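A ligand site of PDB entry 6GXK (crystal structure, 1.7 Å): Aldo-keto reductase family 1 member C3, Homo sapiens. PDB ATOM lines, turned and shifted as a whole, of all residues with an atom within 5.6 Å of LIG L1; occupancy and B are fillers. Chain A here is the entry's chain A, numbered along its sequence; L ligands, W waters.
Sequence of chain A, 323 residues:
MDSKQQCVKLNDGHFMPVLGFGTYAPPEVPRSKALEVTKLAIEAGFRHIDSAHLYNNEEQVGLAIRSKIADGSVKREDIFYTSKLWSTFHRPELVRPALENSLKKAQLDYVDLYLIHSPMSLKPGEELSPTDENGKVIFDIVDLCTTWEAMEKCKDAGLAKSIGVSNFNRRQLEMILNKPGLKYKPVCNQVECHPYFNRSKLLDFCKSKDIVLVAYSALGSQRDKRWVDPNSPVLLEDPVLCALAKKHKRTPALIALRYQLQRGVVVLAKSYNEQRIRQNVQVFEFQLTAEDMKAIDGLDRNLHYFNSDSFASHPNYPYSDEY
O1 of LIG L1 is in hydrogen-bond range of OH of Tyr 55, at 2.6 Å.
NE2 of His 117 lies within hydrogen-bond range of O1 of LIG L1, at 2.7 Å.
An oxygen (O14) of LG2 L2 sits at hydrogen-bond distance from a ring nitrogen (NE2) of His 117, 3.4 Å away.
ND2 of Asn 167 lies within hydrogen-bond range of O14 of LG2 L2, at 2.9 Å.
An oxygen (O10) of LG2 L2 sits at hydrogen-bond distance from the backbone NH of Ser 217 (3.2 Å).
The side-chain hydroxyl (OG) of Ser 217 lies within hydrogen-bond range of an oxygen (O9) of LG2 L2 (2.6 Å).
The backbone NH (N) of Tyr 24 sits at hydrogen-bond distance from an oxygen (O12) of LG2 L2 (3.1 Å).
The backbone NH (N) of Ser 221 lies within hydrogen-bond range of an oxygen (O2) of LG2 L2 (3.0 Å).
The side-chain amide nitrogen of Gln 222 lies within hydrogen-bond range of an oxygen (O8) of LG2 L2 (2.8 Å).
The side-chain hydroxyl (OH) of Tyr 55 sits at hydrogen-bond distance from the side-chain amino group (NZ) of Lys 84, at 3.0 Å.
O of His 117 is in hydrogen-bond range of ND2 of Asn 167 (2.9 Å).
The side-chain hydroxyl (OH) of Tyr 216 lies within hydrogen-bond range of the side-chain amide oxygen (OD1) of Asn 167, at 2.5 Å.
The side-chain hydroxyl (OH) of Tyr 317 sits at hydrogen-bond distance from the side-chain hydroxyl (OG) of Ser 308, 2.9 Å away.
The backbone carbonyl oxygen (O) of Tyr 24 lies within hydrogen-bond range of the side-chain amide nitrogen (NE2) of Gln 222, at 2.8 Å.
The backbone NH (N) of Met 120 sits at hydrogen-bond distance from the side-chain hydroxyl (OG) of Ser 118, 3.1 Å away.
N of Tyr 305 is in hydrogen-bond range of OE2 of Glu 192 (2.9 Å).
Tyr 24 touches LIG L1 (CB to O4, 3.3 Å).
Leu 54 touches LIG L1.
CZ3 of Trp 86 touches C14 of LIG L1 (3.7 Å).
Met 120 touches LIG L1.
CG of Asn 167 touches C11 of LIG L1 (3.2 Å).
OH of Tyr 216 touches C15 of LIG L1, at 3.4 Å.
OG of Ser 217 touches C20 of LIG L1 (3.3 Å).
CB of Ser 221 touches C20 of LIG L1, 3.99 Å away.
Trp 227 touches LIG L1 (CZ3 to N2, 3.9 Å).
Tyr 305 touches LIG L1.
CB of Phe 306 touches C16 of LIG L1, at 3.3 Å.
CB of Ser 308 touches CL1 of LIG L1 (3.5 Å).
Tyr 317 touches LIG L1.
Pro 318 touches LIG L1.
Tyr 319 touches LIG L1.
17 residues have an atom within 4 Å of LIG L1: Tyr 24, Leu 54, Tyr 55, Trp 86, His 117, Met 120, Asn 167, Tyr 216, Ser 217, Ser 221, Trp 227, Tyr 305, Phe 306, Ser 308, Tyr 317, Pro 318 and Tyr 319.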
ATOM      1  N   TYR A  24      -1.334  38.142  25.127  1.00  0.00           N
ATOM      2  CA  TYR A  24      -1.179  37.235  23.994  1.00  0.00           C
ATOM      3  C   TYR A  24      -2.532  36.913  23.374  1.00  0.00           C
ATOM      4  O   TYR A  24      -3.501  36.599  24.074  1.00  0.00           O
ATOM      5  CB  TYR A  24      -0.512  35.911  24.388  1.00  0.00           C
ATOM      6  CG  TYR A  24      -0.391  35.036  23.157  1.00  0.00           C
ATOM      7  CD1 TYR A  24      -1.290  33.999  22.900  1.00  0.00           C
ATOM      8  CD2 TYR A  24       0.572  35.310  22.204  1.00  0.00           C
ATOM      9  CE1 TYR A  24      -1.178  33.228  21.742  1.00  0.00           C
ATOM     10  CE2 TYR A  24       0.680  34.561  21.054  1.00  0.00           C
ATOM     11  CZ  TYR A  24      -0.189  33.529  20.828  1.00  0.00           C
ATOM     12  OH  TYR A  24      -0.060  32.783  19.672  1.00  0.00           O
ATOM     13  N   ALA A  52       5.520  40.675  24.980  1.00  0.00           N
ATOM     14  CA  ALA A  52       6.722  39.925  24.612  1.00  0.00           C
ATOM     15  C   ALA A  52       6.981  40.178  23.130  1.00  0.00           C
ATOM     16  O   ALA A  52       6.046  40.440  22.369  1.00  0.00           O
ATOM     17  CB  ALA A  52       6.561  38.410  24.856  1.00  0.00           C
ATOM     18  N   LEU A  54       7.625  37.857  21.155  1.00  0.00           N
ATOM     19  CA  LEU A  54       6.962  36.750  20.488  1.00  0.00           C
ATOM     20  C   LEU A  54       5.527  37.094  20.081  1.00  0.00           C
ATOM     21  O   LEU A  54       5.010  36.544  19.106  1.00  0.00           O
ATOM     22  CB  LEU A  54       6.950  35.537  21.410  1.00  0.00           C
ATOM     23  CG  LEU A  54       6.301  34.271  20.858  1.00  0.00           C
ATOM     24  CD1 LEU A  54       7.198  33.671  19.768  1.00  0.00           C
ATOM     25  CD2 LEU A  54       6.050  33.243  21.994  1.00  0.00           C
ATOM     26  N   TYR A  55       4.870  37.973  20.827  1.00  0.00           N
ATOM     27  CA  TYR A  55       3.420  38.120  20.686  1.00  0.00           C
ATOM     28  C   TYR A  55       3.015  38.957  19.475  1.00  0.00           C
ATOM     29  O   TYR A  55       1.814  39.064  19.197  1.00  0.00           O
ATOM     30  CB  TYR A  55       2.816  38.757  21.944  1.00  0.00           C
ATOM     31  CG  TYR A  55       3.075  38.009  23.236  1.00  0.00           C
ATOM     32  CD1 TYR A  55       3.590  36.713  23.230  1.00  0.00           C
ATOM     33  CD2 TYR A  55       2.810  38.603  24.473  1.00  0.00           C
ATOM     34  CE1 TYR A  55       3.835  36.032  24.392  1.00  0.00           C
ATOM     35  CE2 TYR A  55       3.036  37.931  25.657  1.00  0.00           C
ATOM     36  CZ  TYR A  55       3.563  36.644  25.602  1.00  0.00           C
ATOM     37  OH  TYR A  55       3.830  35.966  26.758  1.00  0.00           O
ATOM     38  N   LYS A  84       9.673  40.495  26.897  1.00  0.00           N
ATOM     39  CA  LYS A  84      10.447  39.271  27.062  1.00  0.00           C
ATOM     40  C   LYS A  84      11.380  39.065  25.881  1.00  0.00           C
ATOM     41  O   LYS A  84      11.007  39.300  24.725  1.00  0.00           O
ATOM     42  CB  LYS A  84       9.540  38.038  27.200  1.00  0.00           C
ATOM     43  CG  LYS A  84       8.379  38.218  28.194  1.00  0.00           C
ATOM     44  CD  LYS A  84       7.653  36.884  28.435  1.00  0.00           C
ATOM     45  CE  LYS A  84       6.415  37.079  29.300  1.00  0.00           C
ATOM     46  NZ  LYS A  84       5.337  37.817  28.591  1.00  0.00           N
ATOM     47  N   TRP A  86      13.082  36.773  23.319  1.00  0.00           N
ATOM     48  CA  TRP A  86      12.760  35.498  22.719  1.00  0.00           C
ATOM     49  C   TRP A  86      14.010  34.614  22.660  1.00  0.00           C
ATOM     50  O   TRP A  86      15.148  35.090  22.683  1.00  0.00           O
ATOM     51  CB  TRP A  86      12.132  35.680  21.337  1.00  0.00           C
ATOM     52  CG  TRP A  86      11.696  34.355  20.758  1.00  0.00           C
ATOM     53  CD1 TRP A  86      12.093  33.808  19.578  1.00  0.00           C
ATOM     54  CD2 TRP A  86      10.840  33.385  21.375  1.00  0.00           C
ATOM     55  NE1 TRP A  86      11.538  32.572  19.401  1.00  0.00           N
ATOM     56  CE2 TRP A  86      10.755  32.288  20.501  1.00  0.00           C
ATOM     57  CE3 TRP A  86      10.121  33.353  22.585  1.00  0.00           C
ATOM     58  CZ2 TRP A  86       9.981  31.158  20.780  1.00  0.00           C
ATOM     59  CZ3 TRP A  86       9.357  32.221  22.864  1.00  0.00           C
ATOM     60  CH2 TRP A  86       9.295  31.136  21.963  1.00  0.00           C
ATOM     61  N   HIS A 117      12.370  34.799  28.170  1.00  0.00           N
ATOM     62  CA  HIS A 117      11.065  34.159  27.957  1.00  0.00           C
ATOM     63  C   HIS A 117      11.098  32.697  28.347  1.00  0.00           C
ATOM     64  O   HIS A 117      10.095  32.169  28.850  1.00  0.00           O
ATOM     65  CB  HIS A 117      10.643  34.290  26.492  1.00  0.00           C
ATOM     66  CG  HIS A 117       9.158  34.229  26.253  1.00  0.00           C
ATOM     67  ND1 HIS A 117       8.541  35.047  25.339  1.00  0.00           N
ATOM     68  CD2 HIS A 117       8.184  33.459  26.792  1.00  0.00           C
ATOM     69  CE1 HIS A 117       7.245  34.786  25.324  1.00  0.00           C
ATOM     70  NE2 HIS A 117       6.991  33.820  26.188  1.00  0.00           N
ATOM     71  N   SER A 118      12.226  32.036  28.126  1.00  0.00           N
ATOM     72  CA  SER A 118      12.326  30.592  28.335  1.00  0.00           C
ATOM     73  C   SER A 118      13.789  30.216  28.400  1.00  0.00           C
ATOM     74  O   SER A 118      14.626  30.865  27.760  1.00  0.00           O
ATOM     75  CB  SER A 118      11.630  29.819  27.207  1.00  0.00           C
ATOM     76  OG  SER A 118      11.972  28.441  27.231  1.00  0.00           O
ATOM     77  N   MET A 120      14.926  27.614  27.027  1.00  0.00           N
ATOM     78  CA  MET A 120      15.153  26.665  25.942  1.00  0.00           C
ATOM     79  C   MET A 120      15.636  27.393  24.687  1.00  0.00           C
ATOM     80  O   MET A 120      14.888  27.660  23.749  1.00  0.00           O
ATOM     81  CB  MET A 120      13.891  25.845  25.686  1.00  0.00           C
ATOM     82  CG  MET A 120      13.654  24.880  26.821  1.00  0.00           C
ATOM     83  SD  MET A 120      12.334  23.693  26.509  1.00  0.00           S
ATOM     84  CE  MET A 120      10.870  24.725  26.574  1.00  0.00           C
ATOM     85  N   ASN A 167       9.705  30.545  32.962  1.00  0.00           N
ATOM     86  CA  ASN A 167       9.763  29.108  32.651  1.00  0.00           C
ATOM     87  C   ASN A 167      11.037  28.456  33.154  1.00  0.00           C
ATOM     88  O   ASN A 167      11.465  27.433  32.615  1.00  0.00           O
ATOM     89  CB  ASN A 167       9.569  28.880  31.154  1.00  0.00           C
ATOM     90  CG  ASN A 167       8.167  29.275  30.675  1.00  0.00           C
ATOM     91  OD1 ASN A 167       7.176  28.752  31.171  1.00  0.00           O
ATOM     92  ND2 ASN A 167       8.097  30.202  29.725  1.00  0.00           N
ATOM     93  N   GLU A 192       3.912  28.722  34.357  1.00  0.00           N
ATOM     94  CA  GLU A 192       2.530  28.250  34.306  1.00  0.00           C
ATOM     95  C   GLU A 192       2.065  27.897  35.708  1.00  0.00           C
ATOM     96  O   GLU A 192       2.730  27.145  36.430  1.00  0.00           O
ATOM     97  CB  GLU A 192       2.401  27.044  33.385  1.00  0.00           C
ATOM     98  CG  GLU A 192       0.954  26.599  33.206  1.00  0.00           C
ATOM     99  CD  GLU A 192       0.809  25.416  32.294  1.00  0.00           C
ATOM    100  OE1 GLU A 192       1.794  25.056  31.619  1.00  0.00           O
ATOM    101  OE2 GLU A 192      -0.301  24.834  32.248  1.00  0.00           O
ATOM    102  N   TYR A 216       1.225  32.514  34.876  1.00  0.00           N
ATOM    103  CA  TYR A 216       0.499  32.582  33.615  1.00  0.00           C
ATOM    104  C   TYR A 216      -0.363  31.349  33.421  1.00  0.00           C
ATOM    105  O   TYR A 216      -0.218  30.321  34.115  1.00  0.00           O
ATOM    106  CB  TYR A 216       1.429  32.785  32.413  1.00  0.00           C
ATOM    107  CG  TYR A 216       2.293  31.607  31.982  1.00  0.00           C
ATOM    108  CD1 TYR A 216       3.676  31.664  32.110  1.00  0.00           C
ATOM    109  CD2 TYR A 216       1.736  30.477  31.381  1.00  0.00           C
ATOM    110  CE1 TYR A 216       4.478  30.629  31.676  1.00  0.00           C
ATOM    111  CE2 TYR A 216       2.535  29.428  30.959  1.00  0.00           C
ATOM    112  CZ  TYR A 216       3.904  29.515  31.104  1.00  0.00           C
ATOM    113  OH  TYR A 216       4.707  28.480  30.683  1.00  0.00           O
ATOM    114  N   SER A 217      -1.263  31.479  32.451  1.00  0.00           N
ATOM    115  CA  SER A 217      -2.361  30.519  32.216  1.00  0.00           C
ATOM    116  C   SER A 217      -3.073  30.200  33.528  1.00  0.00           C
ATOM    117  O   SER A 217      -3.526  29.083  33.769  1.00  0.00           O
ATOM    118  CB  SER A 217      -1.861  29.256  31.524  1.00  0.00           C
ATOM    119  OG  SER A 217      -1.367  29.564  30.218  1.00  0.00           O
ATOM    120  N   SER A 221      -5.418  28.658  30.452  1.00  0.00           N
ATOM    121  CA  SER A 221      -4.892  28.875  29.111  1.00  0.00           C
ATOM    122  C   SER A 221      -5.984  29.109  28.087  1.00  0.00           C
ATOM    123  O   SER A 221      -7.175  28.970  28.384  1.00  0.00           O
ATOM    124  CB  SER A 221      -3.993  27.713  28.647  1.00  0.00           C
ATOM    125  OG  SER A 221      -4.752  26.689  28.020  1.00  0.00           O
ATOM    126  N   GLN A 222      -5.593  29.511  26.879  1.00  0.00           N
ATOM    127  CA  GLN A 222      -6.543  29.783  25.813  1.00  0.00           C
ATOM    128  C   GLN A 222      -6.910  28.526  25.051  1.00  0.00           C
ATOM    129  O   GLN A 222      -7.711  28.602  24.108  1.00  0.00           O
ATOM    130  CB  GLN A 222      -5.985  30.871  24.877  1.00  0.00           C
ATOM    131  CG  GLN A 222      -5.467  32.065  25.653  1.00  0.00           C
ATOM    132  CD  GLN A 222      -5.157  33.288  24.777  1.00  0.00           C
ATOM    133  OE1 GLN A 222      -5.784  33.495  23.738  1.00  0.00           O
ATOM    134  NE2 GLN A 222      -4.190  34.083  25.206  1.00  0.00           N
ATOM    135  N   TRP A 227      -1.650  23.603  20.326  1.00  0.00           N
ATOM    136  CA  TRP A 227      -0.797  23.364  21.483  1.00  0.00           C
ATOM    137  C   TRP A 227      -1.451  22.550  22.590  1.00  0.00           C
ATOM    138  O   TRP A 227      -0.743  21.901  23.351  1.00  0.00           O
ATOM    139  CB  TRP A 227      -0.338  24.702  22.100  1.00  0.00           C
ATOM    140  CG  TRP A 227       0.355  25.657  21.184  1.00  0.00           C
ATOM    141  CD1 TRP A 227       1.011  25.357  20.021  1.00  0.00           C
ATOM    142  CD2 TRP A 227       0.488  27.072  21.364  1.00  0.00           C
ATOM    143  NE1 TRP A 227       1.535  26.501  19.473  1.00  0.00           N
ATOM    144  CE2 TRP A 227       1.225  27.567  20.281  1.00  0.00           C
ATOM    145  CE3 TRP A 227       0.045  27.960  22.352  1.00  0.00           C
ATOM    146  CZ2 TRP A 227       1.535  28.923  20.142  1.00  0.00           C
ATOM    147  CZ3 TRP A 227       0.342  29.305  22.211  1.00  0.00           C
ATOM    148  CH2 TRP A 227       1.094  29.776  21.119  1.00  0.00           C
ATOM    149  N   TYR A 305      -0.663  22.781  30.300  1.00  0.00           N
ATOM    150  CA  TYR A 305      -1.618  22.890  29.213  1.00  0.00           C
ATOM    151  C   TYR A 305      -0.960  22.820  27.836  1.00  0.00           C
ATOM    152  O   TYR A 305      -1.645  22.481  26.860  1.00  0.00           O
ATOM    153  CB  TYR A 305      -2.471  24.148  29.396  1.00  0.00           C
ATOM    154  CG  TYR A 305      -3.672  23.860  30.283  1.00  0.00           C
ATOM    155  CD1 TYR A 305      -3.767  24.389  31.570  1.00  0.00           C
ATOM    156  CD2 TYR A 305      -4.674  22.999  29.861  1.00  0.00           C
ATOM    157  CE1 TYR A 305      -4.861  24.120  32.398  1.00  0.00           C
ATOM    158  CE2 TYR A 305      -5.772  22.709  30.680  1.00  0.00           C
ATOM    159  CZ  TYR A 305      -5.850  23.273  31.949  1.00  0.00           C
ATOM    160  OH  TYR A 305      -6.937  22.989  32.762  1.00  0.00           O
ATOM    161  N   PHE A 306       0.341  23.048  27.735  1.00  0.00           N
ATOM    162  CA  PHE A 306       1.050  23.074  26.454  1.00  0.00           C
ATOM    163  C   PHE A 306       1.665  21.709  26.176  1.00  0.00           C
ATOM    164  O   PHE A 306       2.397  21.173  26.997  1.00  0.00           O
ATOM    165  CB  PHE A 306       2.144  24.147  26.507  1.00  0.00           C
ATOM    166  CG  PHE A 306       2.844  24.411  25.190  1.00  0.00           C
ATOM    167  CD1 PHE A 306       3.915  23.620  24.785  1.00  0.00           C
ATOM    168  CD2 PHE A 306       2.475  25.482  24.406  1.00  0.00           C
ATOM    169  CE1 PHE A 306       4.570  23.876  23.586  1.00  0.00           C
ATOM    170  CE2 PHE A 306       3.132  25.745  23.201  1.00  0.00           C
ATOM    171  CZ  PHE A 306       4.169  24.940  22.801  1.00  0.00           C
ATOM    172  N   SER A 308       4.350  19.695  25.162  1.00  0.00           N
ATOM    173  CA  SER A 308       5.773  20.018  25.081  1.00  0.00           C
ATOM    174  C   SER A 308       6.617  18.841  24.599  1.00  0.00           C
ATOM    175  O   SER A 308       7.844  18.844  24.810  1.00  0.00           O
ATOM    176  CB  SER A 308       6.276  20.528  26.428  1.00  0.00           C
ATOM    177  OG  SER A 308       5.994  19.583  27.450  1.00  0.00           O
ATOM    178  N   PHE A 311       9.720  19.521  22.666  1.00  0.00           N
ATOM    179  CA  PHE A 311      10.787  20.184  23.406  1.00  0.00           C
ATOM    180  C   PHE A 311      11.332  19.331  24.541  1.00  0.00           C
ATOM    181  O   PHE A 311      12.294  19.743  25.192  1.00  0.00           O
ATOM    182  CB  PHE A 311      10.296  21.526  23.942  1.00  0.00           C
ATOM    183  CG  PHE A 311      10.368  22.638  22.949  1.00  0.00           C
ATOM    184  CD1 PHE A 311       9.276  22.979  22.176  1.00  0.00           C
ATOM    185  CD2 PHE A 311      11.551  23.350  22.760  1.00  0.00           C
ATOM    186  CE1 PHE A 311       9.338  23.999  21.246  1.00  0.00           C
ATOM    187  CE2 PHE A 311      11.634  24.373  21.838  1.00  0.00           C
ATOM    188  CZ  PHE A 311      10.528  24.701  21.078  1.00  0.00           C
ATOM    189  N   TYR A 317      15.000  21.803  28.943  1.00  0.00           N
ATOM    190  CA  TYR A 317      13.613  21.474  29.231  1.00  0.00           C
ATOM    191  C   TYR A 317      13.369  21.572  30.737  1.00  0.00           C
ATOM    192  O   TYR A 317      14.060  20.895  31.524  1.00  0.00           O
ATOM    193  CB  TYR A 317      13.291  20.066  28.726  1.00  0.00           C
ATOM    194  CG  TYR A 317      11.857  19.651  28.884  1.00  0.00           C
ATOM    195  CD1 TYR A 317      10.826  20.330  28.243  1.00  0.00           C
ATOM    196  CD2 TYR A 317      11.519  18.532  29.654  1.00  0.00           C
ATOM    197  CE1 TYR A 317       9.508  19.927  28.384  1.00  0.00           C
ATOM    198  CE2 TYR A 317      10.212  18.133  29.803  1.00  0.00           C
ATOM    199  CZ  TYR A 317       9.215  18.825  29.171  1.00  0.00           C
ATOM    200  OH  TYR A 317       7.912  18.404  29.326  1.00  0.00           O
ATOM    201  N   PRO A 318      12.427  22.396  31.184  1.00  0.00           N
ATOM    202  CA  PRO A 318      12.308  22.684  32.619  1.00  0.00           C
ATOM    203  C   PRO A 318      11.573  21.625  33.432  1.00  0.00           C
ATOM    204  O   PRO A 318      11.669  21.667  34.667  1.00  0.00           O
ATOM    205  CB  PRO A 318      11.534  24.013  32.641  1.00  0.00           C
ATOM    206  CG  PRO A 318      10.751  24.008  31.372  1.00  0.00           C
ATOM    207  CD  PRO A 318      11.666  23.359  30.371  1.00  0.00           C
ATOM    208  N   TYR A 319      10.865  20.691  32.800  1.00  0.00           N
ATOM    209  CA  TYR A 319       9.931  19.836  33.532  1.00  0.00           C
ATOM    210  C   TYR A 319      10.435  18.408  33.713  1.00  0.00           C
ATOM    211  O   TYR A 319       9.622  17.516  33.948  1.00  0.00           O
ATOM    212  CB  TYR A 319       8.575  19.819  32.847  1.00  0.00           C
ATOM    213  CG  TYR A 319       7.839  21.131  32.811  1.00  0.00           C
ATOM    214  CD1 TYR A 319       7.867  22.025  33.886  1.00  0.00           C
ATOM    215  CD2 TYR A 319       7.102  21.486  31.696  1.00  0.00           C
ATOM    216  CE1 TYR A 319       7.177  23.220  33.834  1.00  0.00           C
ATOM    217  CE2 TYR A 319       6.403  22.683  31.645  1.00  0.00           C
ATOM    218  CZ  TYR A 319       6.443  23.539  32.709  1.00  0.00           C
ATOM    219  OH  TYR A 319       5.754  24.736  32.629  1.00  0.00           O
HETATM  220  C1  LIG L   1       2.961  33.202  25.718  1.00  0.00           C
HETATM  221  C2  LIG L   1       3.533  31.145  24.268  1.00  0.00           C
HETATM  222  C3  LIG L   1       4.077  30.086  25.208  1.00  0.00           C
HETATM  223  C4  LIG L   1       3.381  29.156  26.026  1.00  0.00           C
HETATM  224  C5  LIG L   1       5.409  29.820  25.334  1.00  0.00           C
HETATM  225  C6  LIG L   1       4.341  28.387  26.635  1.00  0.00           C
HETATM  226  N1  LIG L   1       5.555  28.806  26.187  1.00  0.00           N
HETATM  227  C7  LIG L   1       2.013  28.956  26.297  1.00  0.00           C
HETATM  228  C8  LIG L   1       1.629  27.959  27.183  1.00  0.00           C
HETATM  229  C9  LIG L   1       6.851  28.345  26.607  1.00  0.00           C
HETATM  230  C10 LIG L   1       6.699  26.065  26.627  1.00  0.00           C
HETATM  231  C11 LIG L   1       8.003  26.897  28.477  1.00  0.00           C
HETATM  232  C12 LIG L   1       6.909  24.757  26.980  1.00  0.00           C
HETATM  233  C13 LIG L   1       2.563  32.086  24.924  1.00  0.00           C
HETATM  234  C14 LIG L   1       6.451  30.648  24.568  1.00  0.00           C
HETATM  235  C15 LIG L   1       3.942  27.370  27.541  1.00  0.00           C
HETATM  236  C16 LIG L   1       2.585  27.175  27.806  1.00  0.00           C
HETATM  237  C17 LIG L   1       7.175  27.116  27.397  1.00  0.00           C
HETATM  238  C18 LIG L   1       8.210  25.573  28.856  1.00  0.00           C
HETATM  239  C19 LIG L   1       7.666  24.542  28.108  1.00  0.00           C
HETATM  240  C20 LIG L   1      -0.065  27.039  28.573  1.00  0.00           C
HETATM  241  N2  LIG L   1       1.232  32.083  24.873  1.00  0.00           N
HETATM  242  N3  LIG L   1       1.836  33.789  26.102  1.00  0.00           N
HETATM  243  O1  LIG L   1       4.271  33.543  26.018  1.00  0.00           O
HETATM  244  O2  LIG L   1       7.825  28.791  26.111  1.00  0.00           O
HETATM  245  O3  LIG L   1       0.265  27.775  27.428  1.00  0.00           O
HETATM  246  O4  LIG L   1       0.823  33.106  25.589  1.00  0.00           O
HETATM  247 CL1  LIG L   1       7.943  22.841  28.534  1.00  0.00          CL
HETATM  248  P1  LG2 L   2      -5.419  32.923  30.767  1.00  0.00           P
HETATM  249  O1  LG2 L   2      -5.083  34.177  31.564  1.00  0.00           O
HETATM  250  O2  LG2 L   2      -5.201  31.569  31.286  1.00  0.00           O
HETATM  251  O3  LG2 L   2      -6.982  33.148  30.387  1.00  0.00           O
HETATM  252  C1  LG2 L   2      -7.320  32.114  29.503  1.00  0.00           C
HETATM  253  C2  LG2 L   2      -8.729  32.423  28.952  1.00  0.00           C
HETATM  254  O4  LG2 L   2      -9.594  32.748  30.025  1.00  0.00           O
HETATM  255  C3  LG2 L   2      -8.640  33.663  28.021  1.00  0.00           C
HETATM  256  O5  LG2 L   2      -8.554  33.272  26.675  1.00  0.00           O
HETATM  257  C4  LG2 L   2     -10.022  34.377  28.266  1.00  0.00           C
HETATM  258  O6  LG2 L   2     -10.845  34.295  27.195  1.00  0.00           O
HETATM  259  C5  LG2 L   2     -10.634  33.573  29.475  1.00  0.00           C
HETATM  260  N1  LG2 L   2     -11.103  34.440  30.523  1.00  0.00           N
HETATM  261  C6  LG2 L   2     -10.485  35.609  31.017  1.00  0.00           C
HETATM  262  N2  LG2 L   2     -11.181  36.188  32.025  1.00  0.00           N
HETATM  263  C7  LG2 L   2     -12.295  35.363  32.164  1.00  0.00           C
HETATM  264  C8  LG2 L   2     -13.387  35.431  33.029  1.00  0.00           C
HETATM  265  N3  LG2 L   2     -13.508  36.430  33.952  1.00  0.00           N
HETATM  266  N4  LG2 L   2     -14.384  34.475  32.983  1.00  0.00           N
HETATM  267  C9  LG2 L   2     -14.208  33.494  32.050  1.00  0.00           C
HETATM  268  N5  LG2 L   2     -13.215  33.299  31.148  1.00  0.00           N
HETATM  269  C10 LG2 L   2     -12.256  34.272  31.252  1.00  0.00           C
HETATM  270  O7  LG2 L   2      -4.678  33.084  29.307  1.00  0.00           O
HETATM  271  P2  LG2 L   2      -3.134  32.866  28.905  1.00  0.00           P
HETATM  272  O8  LG2 L   2      -2.923  33.710  27.729  1.00  0.00           O
HETATM  273  O9  LG2 L   2      -2.750  31.394  28.907  1.00  0.00           O
HETATM  274  O10 LG2 L   2      -2.122  33.498  30.173  1.00  0.00           O
HETATM  275  C11 LG2 L   2      -2.332  34.877  30.217  1.00  0.00           C
HETATM  276  C12 LG2 L   2      -1.042  35.649  29.845  1.00  0.00           C
HETATM  277  O11 LG2 L   2       0.118  35.042  30.433  1.00  0.00           O
HETATM  278  C13 LG2 L   2      -0.771  35.575  28.327  1.00  0.00           C
HETATM  279  O12 LG2 L   2      -1.666  36.451  27.672  1.00  0.00           O
HETATM  280  C14 LG2 L   2       0.660  36.079  28.319  1.00  0.00           C
HETATM  281  O13 LG2 L   2       0.704  37.465  28.614  1.00  0.00           O
HETATM  282  C15 LG2 L   2       1.233  35.316  29.584  1.00  0.00           C
HETATM  283  N6  LG2 L   2       1.860  33.995  29.204  1.00  0.00           N
HETATM  284  C16 LG2 L   2       3.232  33.862  29.294  1.00  0.00           C
HETATM  285  C17 LG2 L   2       3.822  32.654  28.957  1.00  0.00           C
HETATM  286  C18 LG2 L   2       5.271  32.501  29.076  1.00  0.00           C
HETATM  287  O14 LG2 L   2       5.865  31.579  28.545  1.00  0.00           O
HETATM  288  N7  LG2 L   2       5.968  33.393  29.860  1.00  0.00           N
HETATM  289  C19 LG2 L   2       3.039  31.580  28.517  1.00  0.00           C
HETATM  290  C20 LG2 L   2       1.647  31.716  28.441  1.00  0.00           C
HETATM  291  C21 LG2 L   2       1.065  32.913  28.798  1.00  0.00           C
HETATM  292  P3  LG2 L   2     -11.545  35.778  26.508  1.00  0.00           P
HETATM  293  O15 LG2 L   2     -10.307  36.440  25.961  1.00  0.00           O
HETATM  294  O16 LG2 L   2     -12.593  35.284  25.549  1.00  0.00           O
HETATM  295  O17 LG2 L   2     -11.969  36.444  27.803  1.00  0.00           O
HETATM  296  O   HOH W   1      -1.519  26.764  25.568  1.00  0.00           O
